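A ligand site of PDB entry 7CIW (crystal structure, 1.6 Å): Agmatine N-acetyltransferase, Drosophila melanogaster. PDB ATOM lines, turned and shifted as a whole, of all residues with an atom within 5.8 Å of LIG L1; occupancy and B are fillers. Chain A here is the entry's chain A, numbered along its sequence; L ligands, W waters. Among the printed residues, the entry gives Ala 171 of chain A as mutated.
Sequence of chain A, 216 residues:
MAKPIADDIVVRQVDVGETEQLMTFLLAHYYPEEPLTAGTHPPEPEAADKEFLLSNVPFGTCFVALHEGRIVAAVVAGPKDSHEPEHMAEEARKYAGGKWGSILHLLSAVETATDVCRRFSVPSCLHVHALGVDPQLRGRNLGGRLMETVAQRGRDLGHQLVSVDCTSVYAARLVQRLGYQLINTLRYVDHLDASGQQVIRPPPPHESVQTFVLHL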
ATOM      1  N   HIS A  29      -6.091  35.123 -14.265  1.00  0.00           N
ATOM      2  CA  HIS A  29      -5.414  33.952 -14.804  1.00  0.00           C
ATOM      3  C   HIS A  29      -6.336  32.927 -15.457  1.00  0.00           C
ATOM      4  O   HIS A  29      -5.833  31.936 -15.986  1.00  0.00           O
ATOM      5  CB  HIS A  29      -4.603  33.257 -13.690  1.00  0.00           C
ATOM      6  CG  HIS A  29      -3.515  34.115 -13.147  1.00  0.00           C
ATOM      7  ND1 HIS A  29      -2.563  34.716 -13.946  1.00  0.00           N
ATOM      8  CD2 HIS A  29      -3.223  34.490 -11.874  1.00  0.00           C
ATOM      9  CE1 HIS A  29      -1.731  35.417 -13.199  1.00  0.00           C
ATOM     10  NE2 HIS A  29      -2.113  35.299 -11.940  1.00  0.00           N
ATOM     11  N   TYR A  30      -7.641  33.135 -15.419  1.00  0.00           N
ATOM     12  CA  TYR A  30      -8.580  32.262 -16.115  1.00  0.00           C
ATOM     13  C   TYR A  30      -9.147  32.956 -17.340  1.00  0.00           C
ATOM     14  O   TYR A  30      -8.899  32.518 -18.476  1.00  0.00           O
ATOM     15  CB  TYR A  30      -9.708  31.824 -15.174  1.00  0.00           C
ATOM     16  CG  TYR A  30     -10.821  31.085 -15.888  1.00  0.00           C
ATOM     17  CD1 TYR A  30     -10.640  29.769 -16.316  1.00  0.00           C
ATOM     18  CD2 TYR A  30     -12.050  31.690 -16.120  1.00  0.00           C
ATOM     19  CE1 TYR A  30     -11.649  29.092 -16.971  1.00  0.00           C
ATOM     20  CE2 TYR A  30     -13.073  31.017 -16.778  1.00  0.00           C
ATOM     21  CZ  TYR A  30     -12.853  29.713 -17.194  1.00  0.00           C
ATOM     22  OH  TYR A  30     -13.868  29.048 -17.843  1.00  0.00           O
ATOM     23  N   TYR A  31      -9.881  34.036 -17.131  1.00  0.00           N
ATOM     24  CA  TYR A  31     -10.577  34.699 -18.227  1.00  0.00           C
ATOM     25  C   TYR A  31      -9.664  35.193 -19.358  1.00  0.00           C
ATOM     26  O   TYR A  31     -10.069  35.080 -20.523  1.00  0.00           O
ATOM     27  CB  TYR A  31     -11.384  35.865 -17.664  1.00  0.00           C
ATOM     28  CG  TYR A  31     -12.724  35.521 -17.054  1.00  0.00           C
ATOM     29  CD1 TYR A  31     -13.760  35.016 -17.834  1.00  0.00           C
ATOM     30  CD2 TYR A  31     -12.971  35.771 -15.716  1.00  0.00           C
ATOM     31  CE1 TYR A  31     -15.016  34.750 -17.279  1.00  0.00           C
ATOM     32  CE2 TYR A  31     -14.222  35.521 -15.155  1.00  0.00           C
ATOM     33  CZ  TYR A  31     -15.239  35.021 -15.944  1.00  0.00           C
ATOM     34  OH  TYR A  31     -16.475  34.784 -15.396  1.00  0.00           O
ATOM     35  N   GLU A  33      -7.125  33.963 -20.803  1.00  0.00           N
ATOM     36  CA  GLU A  33      -6.643  32.894 -21.673  1.00  0.00           C
ATOM     37  C   GLU A  33      -7.705  31.842 -21.998  1.00  0.00           C
ATOM     38  O   GLU A  33      -7.476  31.027 -22.905  1.00  0.00           O
ATOM     39  CB  GLU A  33      -5.433  32.195 -21.039  1.00  0.00           C
ATOM     40  CG  GLU A  33      -4.297  33.138 -20.720  1.00  0.00           C
ATOM     41  CD  GLU A  33      -3.260  32.502 -19.815  1.00  0.00           C
ATOM     42  OE1 GLU A  33      -2.535  31.601 -20.297  1.00  0.00           O
ATOM     43  OE2 GLU A  33      -3.196  32.888 -18.623  1.00  0.00           O
ATOM     44  N   GLU A  34      -8.831  31.841 -21.319  1.00  0.00           N
ATOM     45  CA  GLU A  34      -9.888  30.893 -21.656  1.00  0.00           C
ATOM     46  C   GLU A  34     -10.359  31.150 -23.083  1.00  0.00           C
ATOM     47  O   GLU A  34     -10.683  32.294 -23.429  1.00  0.00           O
ATOM     48  CB  GLU A  34     -11.040  31.019 -20.662  1.00  0.00           C
ATOM     49  CG  GLU A  34     -12.040  29.885 -20.769  1.00  0.00           C
ATOM     50  CD  GLU A  34     -13.013  30.106 -21.899  1.00  0.00           C
ATOM     51  OE1 GLU A  34     -13.548  31.229 -21.994  1.00  0.00           O
ATOM     52  OE2 GLU A  34     -13.215  29.173 -22.706  1.00  0.00           O
ATOM     53  N   PRO A  35     -10.398  30.132 -23.943  1.00  0.00           N
ATOM     54  CA  PRO A  35     -10.623  30.407 -25.380  1.00  0.00           C
ATOM     55  C   PRO A  35     -11.927  31.121 -25.723  1.00  0.00           C
ATOM     56  O   PRO A  35     -11.901  31.990 -26.606  1.00  0.00           O
ATOM     57  CB  PRO A  35     -10.553  28.997 -25.996  1.00  0.00           C
ATOM     58  CG  PRO A  35      -9.541  28.296 -25.137  1.00  0.00           C
ATOM     59  CD  PRO A  35      -9.832  28.779 -23.724  1.00  0.00           C
ATOM     60  N   LEU A 131     -12.092  26.199 -14.946  1.00  0.00           N
ATOM     61  CA  LEU A 131     -10.869  25.633 -14.377  1.00  0.00           C
ATOM     62  C   LEU A 131      -9.704  26.509 -14.808  1.00  0.00           C
ATOM     63  O   LEU A 131      -9.500  26.699 -16.001  1.00  0.00           O
ATOM     64  CB  LEU A 131     -10.663  24.195 -14.846  1.00  0.00           C
ATOM     65  CG  LEU A 131      -9.433  23.521 -14.260  1.00  0.00           C
ATOM     66  CD1 LEU A 131      -9.655  23.209 -12.795  1.00  0.00           C
ATOM     67  CD2 LEU A 131      -9.137  22.241 -15.056  1.00  0.00           C
ATOM     68  N   GLY A 132      -8.941  27.031 -13.841  1.00  0.00           N
ATOM     69  CA  GLY A 132      -7.784  27.857 -14.183  1.00  0.00           C
ATOM     70  C   GLY A 132      -6.671  27.667 -13.169  1.00  0.00           C
ATOM     71  O   GLY A 132      -6.924  27.415 -11.985  1.00  0.00           O
ATOM     72  N   VAL A 133      -5.432  27.781 -13.645  1.00  0.00           N
ATOM     73  CA  VAL A 133      -4.221  27.663 -12.832  1.00  0.00           C
ATOM     74  C   VAL A 133      -3.325  28.849 -13.142  1.00  0.00           C
ATOM     75  O   VAL A 133      -3.156  29.206 -14.321  1.00  0.00           O
ATOM     76  CB  VAL A 133      -3.482  26.338 -13.096  1.00  0.00           C
ATOM     77  CG1 VAL A 133      -2.182  26.289 -12.304  1.00  0.00           C
ATOM     78  CG2 VAL A 133      -4.351  25.143 -12.694  1.00  0.00           C
ATOM     79  N   ASP A 134      -2.772  29.487 -12.108  1.00  0.00           N
ATOM     80  CA  ASP A 134      -1.772  30.528 -12.258  1.00  0.00           C
ATOM     81  C   ASP A 134      -0.658  30.040 -13.169  1.00  0.00           C
ATOM     82  O   ASP A 134      -0.131  28.934 -12.964  1.00  0.00           O
ATOM     83  CB  ASP A 134      -1.222  30.896 -10.868  1.00  0.00           C
ATOM     84  CG  ASP A 134      -0.292  32.106 -10.871  1.00  0.00           C
ATOM     85  OD1 ASP A 134       0.619  32.210 -11.713  1.00  0.00           O
ATOM     86  OD2 ASP A 134      -0.431  32.943  -9.957  1.00  0.00           O
ATOM     87  N   LEU A 137       2.273  28.241 -11.743  1.00  0.00           N
ATOM     88  CA  LEU A 137       2.070  26.928 -11.135  1.00  0.00           C
ATOM     89  C   LEU A 137       1.593  25.896 -12.154  1.00  0.00           C
ATOM     90  O   LEU A 137       1.188  24.796 -11.743  1.00  0.00           O
ATOM     91  CB  LEU A 137       1.074  27.029  -9.980  1.00  0.00           C
ATOM     92  CG  LEU A 137       1.483  27.554  -8.590  1.00  0.00           C
ATOM     93  CD1 LEU A 137       2.576  26.679  -7.990  1.00  0.00           C
ATOM     94  CD2 LEU A 137       1.910  29.007  -8.624  1.00  0.00           C
ATOM     95  N   ARG A 138       1.607  26.207 -13.437  1.00  0.00           N
ATOM     96  CA  ARG A 138       1.122  25.263 -14.434  1.00  0.00           C
ATOM     97  C   ARG A 138       2.129  24.144 -14.651  1.00  0.00           C
ATOM     98  O   ARG A 138       3.339  24.325 -14.492  1.00  0.00           O
ATOM     99  CB  ARG A 138       0.795  25.963 -15.751  1.00  0.00           C
ATOM    100  CG  ARG A 138      -0.473  26.814 -15.655  1.00  0.00           C
ATOM    101  CD  ARG A 138      -0.825  27.543 -16.933  1.00  0.00           C
ATOM    102  NE  ARG A 138      -1.898  28.498 -16.693  1.00  0.00           N
ATOM    103  CZ  ARG A 138      -2.215  29.508 -17.494  1.00  0.00           C
ATOM    104  NH1 ARG A 138      -1.540  29.685 -18.631  1.00  0.00           N
ATOM    105  NH2 ARG A 138      -3.200  30.325 -17.173  1.00  0.00           N
ATOM    106  N   GLY A 139       1.623  22.970 -14.998  1.00  0.00           N
ATOM    107  CA  GLY A 139       2.474  21.807 -15.171  1.00  0.00           C
ATOM    108  C   GLY A 139       2.771  21.052 -13.894  1.00  0.00           C
ATOM    109  O   GLY A 139       3.657  20.191 -13.885  1.00  0.00           O
ATOM    110  N   ARG A 140       2.048  21.347 -12.815  1.00  0.00           N
ATOM    111  CA  ARG A 140       2.217  20.676 -11.531  1.00  0.00           C
ATOM    112  C   ARG A 140       0.962  19.920 -11.133  1.00  0.00           C
ATOM    113  O   ARG A 140       0.760  19.633  -9.950  1.00  0.00           O
ATOM    114  CB  ARG A 140       2.602  21.669 -10.439  1.00  0.00           C
ATOM    115  CG  ARG A 140       3.604  22.749 -10.847  1.00  0.00           C
ATOM    116  CD  ARG A 140       4.853  22.166 -11.482  1.00  0.00           C
ATOM    117  NE  ARG A 140       5.984  22.100 -10.561  1.00  0.00           N
ATOM    118  CZ  ARG A 140       7.113  21.448 -10.819  1.00  0.00           C
ATOM    119  NH1 ARG A 140       7.260  20.803 -11.966  1.00  0.00           N
ATOM    120  NH2 ARG A 140       8.093  21.443  -9.920  1.00  0.00           N
ATOM    121  N   ASN A 141       0.094  19.618 -12.104  1.00  0.00           N
ATOM    122  CA  ASN A 141      -1.150  18.858 -11.905  1.00  0.00           C
ATOM    123  C   ASN A 141      -2.075  19.508 -10.879  1.00  0.00           C
ATOM    124  O   ASN A 141      -2.857  18.829 -10.209  1.00  0.00           O
ATOM    125  CB  ASN A 141      -0.852  17.398 -11.521  1.00  0.00           C
ATOM    126  CG  ASN A 141      -2.079  16.506 -11.637  1.00  0.00           C
ATOM    127  OD1 ASN A 141      -2.688  16.404 -12.709  1.00  0.00           O
ATOM    128  ND2 ASN A 141      -2.448  15.870 -10.534  1.00  0.00           N
ATOM    129  N   LEU A 142      -2.028  20.831 -10.727  1.00  0.00           N
ATOM    130  CA  LEU A 142      -3.032  21.482  -9.895  1.00  0.00           C
ATOM    131  C   LEU A 142      -4.417  21.386 -10.536  1.00  0.00           C
ATOM    132  O   LEU A 142      -5.429  21.237  -9.833  1.00  0.00           O
ATOM    133  CB  LEU A 142      -2.666  22.950  -9.646  1.00  0.00           C
ATOM    134  CG  LEU A 142      -1.459  23.214  -8.759  1.00  0.00           C
ATOM    135  CD1 LEU A 142      -1.469  24.681  -8.333  1.00  0.00           C
ATOM    136  CD2 LEU A 142      -1.461  22.297  -7.559  1.00  0.00           C
ATOM    137  N   GLY A 143      -4.482  21.489 -11.859  1.00  0.00           N
ATOM    138  CA  GLY A 143      -5.775  21.315 -12.512  1.00  0.00           C
ATOM    139  C   GLY A 143      -6.359  19.937 -12.228  1.00  0.00           C
ATOM    140  O   GLY A 143      -7.528  19.813 -11.856  1.00  0.00           O
ATOM    141  N   GLY A 144      -5.536  18.904 -12.364  1.00  0.00           N
ATOM    142  CA  GLY A 144      -6.022  17.554 -12.096  1.00  0.00           C
ATOM    143  C   GLY A 144      -6.437  17.367 -10.648  1.00  0.00           C
ATOM    144  O   GLY A 144      -7.423  16.694 -10.364  1.00  0.00           O
ATOM    145  N   VAL A 164     -17.592  18.267 -18.533  1.00  0.00           N
ATOM    146  CA  VAL A 164     -16.782  19.475 -18.661  1.00  0.00           C
ATOM    147  C   VAL A 164     -16.594  19.812 -20.140  1.00  0.00           C
ATOM    148  O   VAL A 164     -16.320  18.927 -20.954  1.00  0.00           O
ATOM    149  CB  VAL A 164     -15.438  19.309 -17.919  1.00  0.00           C
ATOM    150  CG1 VAL A 164     -14.651  18.091 -18.467  1.00  0.00           C
ATOM    151  CG2 VAL A 164     -14.597  20.589 -17.992  1.00  0.00           C
ATOM    152  N   ASP A 165     -16.793  21.089 -20.511  1.00  0.00           N
ATOM    153  CA  ASP A 165     -16.563  21.548 -21.886  1.00  0.00           C
ATOM    154  C   ASP A 165     -15.138  22.068 -21.988  1.00  0.00           C
ATOM    155  O   ASP A 165     -14.854  23.197 -21.607  1.00  0.00           O
ATOM    156  CB  ASP A 165     -17.548  22.639 -22.285  1.00  0.00           C
ATOM    157  CG  ASP A 165     -18.995  22.213 -22.186  1.00  0.00           C
ATOM    158  OD1 ASP A 165     -19.300  21.035 -22.490  1.00  0.00           O
ATOM    159  OD2 ASP A 165     -19.838  23.058 -21.820  1.00  0.00           O
ATOM    160  N   CYS A 166     -14.245  21.255 -22.538  1.00  0.00           N
ATOM    161  CA  CYS A 166     -12.851  21.678 -22.698  1.00  0.00           C
ATOM    162  C   CYS A 166     -12.739  22.548 -23.940  1.00  0.00           C
ATOM    163  O   CYS A 166     -12.529  22.074 -25.060  1.00  0.00           O
ATOM    164  CB  CYS A 166     -11.931  20.464 -22.758  1.00  0.00           C
ATOM    165  SG  CYS A 166     -11.912  19.505 -21.221  1.00  0.00           S
ATOM    166  N   THR A 167     -12.912  23.846 -23.739  1.00  0.00           N
ATOM    167  CA  THR A 167     -12.689  24.813 -24.783  1.00  0.00           C
ATOM    168  C   THR A 167     -11.204  24.948 -25.120  1.00  0.00           C
ATOM    169  O   THR A 167     -10.863  25.409 -26.212  1.00  0.00           O
ATOM    170  CB  THR A 167     -13.264  26.166 -24.353  1.00  0.00           C
ATOM    171  OG1 THR A 167     -12.639  26.560 -23.131  1.00  0.00           O
ATOM    172  CG2 THR A 167     -14.763  26.036 -24.105  1.00  0.00           C
ATOM    173  N   SER A 168     -10.341  24.513 -24.213  1.00  0.00           N
ATOM    174  CA  SER A 168      -8.892  24.585 -24.343  1.00  0.00           C
ATOM    175  C   SER A 168      -8.326  23.184 -24.503  1.00  0.00           C
ATOM    176  O   SER A 168      -8.734  22.254 -23.787  1.00  0.00           O
ATOM    177  CB  SER A 168      -8.281  25.243 -23.094  1.00  0.00           C
ATOM    178  OG  SER A 168      -6.910  24.946 -22.964  1.00  0.00           O
ATOM    179  N   TYR A 170      -5.446  22.186 -23.661  1.00  0.00           N
ATOM    180  CA  TYR A 170      -4.718  21.785 -22.455  1.00  0.00           C
ATOM    181  C   TYR A 170      -5.654  21.153 -21.431  1.00  0.00           C
ATOM    182  O   TYR A 170      -5.274  20.219 -20.720  1.00  0.00           O
ATOM    183  CB  TYR A 170      -4.003  22.986 -21.850  1.00  0.00           C
ATOM    184  CG  TYR A 170      -3.141  23.681 -22.865  1.00  0.00           C
ATOM    185  CD1 TYR A 170      -2.100  22.998 -23.499  1.00  0.00           C
ATOM    186  CD2 TYR A 170      -3.360  25.001 -23.222  1.00  0.00           C
ATOM    187  CE1 TYR A 170      -1.318  23.605 -24.433  1.00  0.00           C
ATOM    188  CE2 TYR A 170      -2.576  25.625 -24.171  1.00  0.00           C
ATOM    189  CZ  TYR A 170      -1.552  24.911 -24.777  1.00  0.00           C
ATOM    190  OH  TYR A 170      -0.754  25.508 -25.725  1.00  0.00           O
ATOM    191  N   ALA A 171      -6.879  21.656 -21.341  1.00  0.00           N
ATOM    192  CA  ALA A 171      -7.840  21.030 -20.449  1.00  0.00           C
ATOM    193  C   ALA A 171      -8.283  19.676 -20.994  1.00  0.00           C
ATOM    194  O   ALA A 171      -8.436  18.722 -20.230  1.00  0.00           O
ATOM    195  CB  ALA A 171      -9.038  21.946 -20.216  1.00  0.00           C
ATOM    196  N   LEU A 174      -5.618  17.292 -20.085  1.00  0.00           N
ATOM    197  CA  LEU A 174      -5.664  17.003 -18.654  1.00  0.00           C
ATOM    198  C   LEU A 174      -6.722  15.947 -18.327  1.00  0.00           C
ATOM    199  O   LEU A 174      -6.448  14.981 -17.600  1.00  0.00           O
ATOM    200  CB  LEU A 174      -5.922  18.298 -17.868  1.00  0.00           C
ATOM    201  CG  LEU A 174      -6.410  18.078 -16.443  1.00  0.00           C
ATOM    202  CD1 LEU A 174      -5.290  17.429 -15.638  1.00  0.00           C
ATOM    203  CD2 LEU A 174      -6.853  19.365 -15.779  1.00  0.00           C
ATOM    204  N   ARG A 177      -5.917  12.453 -19.328  1.00  0.00           N
ATOM    205  CA  ARG A 177      -5.027  11.823 -18.352  1.00  0.00           C
ATOM    206  C   ARG A 177      -5.799  11.339 -17.128  1.00  0.00           C
ATOM    207  O   ARG A 177      -5.422  10.341 -16.513  1.00  0.00           O
ATOM    208  CB  ARG A 177      -3.930  12.826 -17.984  1.00  0.00           C
ATOM    209  CG  ARG A 177      -3.340  12.715 -16.599  1.00  0.00           C
ATOM    210  CD  ARG A 177      -2.055  13.528 -16.543  1.00  0.00           C
ATOM    211  NE  ARG A 177      -2.213  14.798 -15.819  1.00  0.00           N
ATOM    212  CZ  ARG A 177      -2.025  16.005 -16.352  1.00  0.00           C
ATOM    213  NH1 ARG A 177      -1.682  16.136 -17.621  1.00  0.00           N
ATOM    214  NH2 ARG A 177      -2.169  17.083 -15.593  1.00  0.00           N
HETATM  215  N1  LIG L   1      -0.282  27.012 -22.148  1.00  0.00           N
HETATM  216  C1  LIG L   1       0.840  26.325 -22.513  1.00  0.00           C
HETATM  217  N2  LIG L   1       1.140  25.118 -21.915  1.00  0.00           N
HETATM  218  C2  LIG L   1       0.341  24.616 -20.965  1.00  0.00           C
HETATM  219  C3  LIG L   1      -0.758  25.300 -20.607  1.00  0.00           C
HETATM  220  C4  LIG L   1      -1.056  26.504 -21.214  1.00  0.00           C
HETATM  221  N3  LIG L   1      -2.123  27.585 -21.164  1.00  0.00           N
HETATM  222  N4  LIG L   1      -1.414  24.614 -19.638  1.00  0.00           N
HETATM  223  C5  LIG L   1      -0.723  23.490 -19.380  1.00  0.00           C
HETATM  224  N5  LIG L   1       0.334  23.496 -20.199  1.00  0.00           N
HETATM  225  C6  LIG L   1       1.387  22.677 -20.371  1.00  0.00           C
HETATM  226  C7  LIG L   1       2.128  22.620 -19.001  1.00  0.00           C
HETATM  227  O1  LIG L   1       3.060  23.759 -18.832  1.00  0.00           O
HETATM  228  C8  LIG L   1       2.717  21.406 -18.963  1.00  0.00           C
HETATM  229  O2  LIG L   1       3.885  21.270 -19.824  1.00  0.00           O
HETATM  230  P1  LIG L   1       5.442  21.517 -19.303  1.00  0.00           P
HETATM  231  O3  LIG L   1       5.572  21.162 -17.833  1.00  0.00           O
HETATM  232  O4  LIG L   1       6.414  20.723 -20.188  1.00  0.00           O
HETATM  233  O5  LIG L   1       5.694  23.011 -19.496  1.00  0.00           O
HETATM  234  C9  LIG L   1       1.629  20.426 -19.689  1.00  0.00           C
HETATM  235  O6  LIG L   1       0.920  21.189 -20.522  1.00  0.00           O
HETATM  236  C10 LIG L   1       0.766  19.713 -18.690  1.00  0.00           C
HETATM  237  O7  LIG L   1       0.381  20.646 -17.686  1.00  0.00           O
HETATM  238  P2  LIG L   1      -0.956  20.369 -16.714  1.00  0.00           P
HETATM  239  O8  LIG L   1      -1.878  19.275 -17.248  1.00  0.00           O
HETATM  240  O9  LIG L   1      -0.489  20.120 -15.291  1.00  0.00           O
HETATM  241  O10 LIG L   1      -1.794  21.781 -16.814  1.00  0.00           O
HETATM  242  P3  LIG L   1      -2.385  22.661 -15.557  1.00  0.00           P
HETATM  243  O11 LIG L   1      -1.263  23.266 -14.776  1.00  0.00           O
HETATM  244  O12 LIG L   1      -3.317  21.811 -14.726  1.00  0.00           O
HETATM  245  O13 LIG L   1      -3.190  23.836 -16.394  1.00  0.00           O
HETATM  246  C11 LIG L   1      -5.149  24.642 -17.338  1.00  0.00           C
HETATM  247  C12 LIG L   1      -4.210  23.459 -17.257  1.00  0.00           C
HETATM  248  C13 LIG L   1      -5.865  24.762 -15.944  1.00  0.00           C
HETATM  249  C14 LIG L   1      -6.178  24.420 -18.446  1.00  0.00           C
HETATM  250  C15 LIG L   1      -4.322  25.879 -17.676  1.00  0.00           C
HETATM  251  O14 LIG L   1      -3.818  25.742 -18.980  1.00  0.00           O
HETATM  252  C16 LIG L   1      -5.105  27.201 -17.598  1.00  0.00           C
HETATM  253  O15 LIG L   1      -5.378  27.737 -16.572  1.00  0.00           O
HETATM  254  N6  LIG L   1      -5.495  27.825 -18.857  1.00  0.00           N
HETATM  255  C17 LIG L   1      -6.199  29.118 -18.886  1.00  0.00           C
HETATM  256  C18 LIG L   1      -7.746  29.045 -18.557  1.00  0.00           C
HETATM  257  C19 LIG L   1      -8.319  27.938 -19.417  1.00  0.00           C
HETATM  258  O16 LIG L   1      -8.177  27.909 -20.610  1.00  0.00           O
HETATM  259  N7  LIG L   1      -9.060  26.871 -18.675  1.00  0.00           N
HETATM  260  C20 LIG L   1      -9.633  25.695 -19.299  1.00  0.00           C
HETATM  261  C21 LIG L   1     -10.809  26.018 -20.228  1.00  0.00           C
HETATM  262  S1  LIG L   1     -11.410  24.346 -20.615  1.00  0.00           S
HETATM  263  C1  LG2 L   2     -17.325  31.696 -19.261  1.00  0.00           C
HETATM  264  N1  LG2 L   2     -16.647  32.732 -20.034  1.00  0.00           N
HETATM  265  C2  LG2 L   2     -13.774  24.173 -17.546  1.00  0.00           C
HETATM  266  C3  LG2 L   2     -13.851  25.468 -18.363  1.00  0.00           C
HETATM  267  C4  LG2 L   2     -14.843  26.724 -20.320  1.00  0.00           C
HETATM  268  C5  LG2 L   2     -16.144  27.482 -20.007  1.00  0.00           C
HETATM  269  C6  LG2 L   2     -16.400  28.642 -20.976  1.00  0.00           C
HETATM  270  C7  LG2 L   2     -16.112  30.045 -20.419  1.00  0.00           C
HETATM  271  N2  LG2 L   2     -14.733  25.521 -19.518  1.00  0.00           N
HETATM  272  N3  LG2 L   2     -17.091  30.481 -19.448  1.00  0.00           N
HETATM  273  N4  LG2 L   2     -18.298  32.073 -18.269  1.00  0.00           N
HETATM  274  O1  LG2 L   2     -13.211  26.407 -18.054  1.00  0.00           O
HETATM  275  O   HOH W   1      -0.669  20.092 -22.224  1.00  0.00           O
HETATM  276  O   HOH W   2       5.224  24.096 -21.933  1.00  0.00           O
HETATM  277  O   HOH W   3      -5.922  27.187 -21.779  1.00  0.00           O
HETATM  278  O   HOH W   4      -0.489  22.776 -12.245  1.00  0.00           O
HETATM  279  O   HOH W   5       8.347  22.116 -21.930  1.00  0.00           O
HETATM  280  O   HOH W   6      -2.689  19.842 -20.066  1.00  0.00           O
HETATM  281  O   HOH W   7       2.557  26.632 -19.132  1.00  0.00           O
HETATM  282  O   HOH W   8      -3.294  19.391 -14.172  1.00  0.00           O
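Water W3 bridges an oxygen (O16) of LIG L1 and the side-chain hydroxyl of Ser 168.
Water W6 lies within hydrogen-bond range of O of Tyr 170 (2.7 Å) and O8 of LIG L1 (3.0 Å).
OD1 of Asn 141 lies within hydrogen-bond range of NH2 of Arg 177, at 3.0 Å.
The backbone carbonyl oxygen (O) of Val 133 is in hydrogen-bond range of the guanidinium group (NE) of Arg 138 (2.8 Å).
The side-chain carboxylate (OE1) of Glu 33 lies within salt-bridge range of the guanidinium group (NH1) of Arg 138, at 2.7 Å.
The backbone carbonyl oxygen of His 29 lies within hydrogen-bond range of the guanidinium group of Arg 138, 3.3 Å away.
The backbone NH (N) of Tyr 170 sits close to the side-chain hydroxyl (OG) of Ser 168 (3.2 Å).
SG of Cys 166 sits close to O of Ala 171, at 3.7 Å.
The side-chain carboxylate (OE2) of Glu 34 sits at hydrogen-bond distance from the side-chain hydroxyl (OG1) of Thr 167, at 2.7 Å.
The backbone carbonyl oxygen (O) of Leu 131 is in hydrogen-bond range of a nitrogen (N7) of LIG L1 (2.7 Å).
O8 of LIG L1 lies within salt-bridge range of NH2 of Arg 177, at 2.8 Å.
N of Gly 139 sits at hydrogen-bond distance from O11 of LIG L1, 2.9 Å away.
N of Val 133 is in hydrogen-bond range of O15 of LIG L1.
O12 of LIG L1 lies within hydrogen-bond range of N of Gly 143.
The guanidinium group (NH2) of Arg 138 is in hydrogen-bond range of an oxygen (O15) of LIG L1 (3.4 Å).
The backbone NH (N) of Asn 141 lies within hydrogen-bond range of an oxygen (O9) of LIG L1 (3.3 Å).
A sulfur (S1) of LIG L1 sits close to the backbone NH (N) of Thr 167 (3.5 Å).
The side-chain hydroxyl (OG1) of Thr 167 sits close to a sulfur (S1) of LIG L1 (3.6 Å).
The backbone NH (N) of Ser 168 lies close to a sulfur (S1) of LIG L1, at 3.8 Å.
O of Asp 165 sits close to S1 of LIG L1 (3.8 Å).
An oxygen (O1) of LG2 L2 is in hydrogen-bond range of the backbone NH (N) of Leu 131, 3.3 Å away.
The side-chain carboxylate (OE1) of Glu 34 lies within salt-bridge range of a nitrogen (N1) of LG2 L2.
O1 of LG2 L2 is in hydrogen-bond range of OH of Tyr 30, 2.7 Å away.
A nitrogen (N2) of LG2 L2 lies within hydrogen-bond range of the backbone carbonyl oxygen (O) of Asp 165.
Merely in contact with LIG L1: Tyr 30 (3.7 Å), Glu 33 (3.8 Å), Glu 34 (3.6 Å), Pro 35 (3.6 Å), Gly 132 (3.4 Å), Arg 140 (3.8 Å), Cys 166 (3.7 Å), Tyr 170 (3.4 Å) and Ala 171 (3.4 Å).
Hydrophobic or aromatic side chains within 4 Å of LIG L1: Tyr 30, Pro 35, Val 133, Tyr 170 and Ala 171.
Along chain A the residues within 4 Å of LIG L1 span positions 30 to 177.
The nearest printed residue that does not touch LIG L1 is His 29 (4.1 Å).
S1 of LIG L1 sits close to N2 of LG2 L2, 3.7 Å away.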
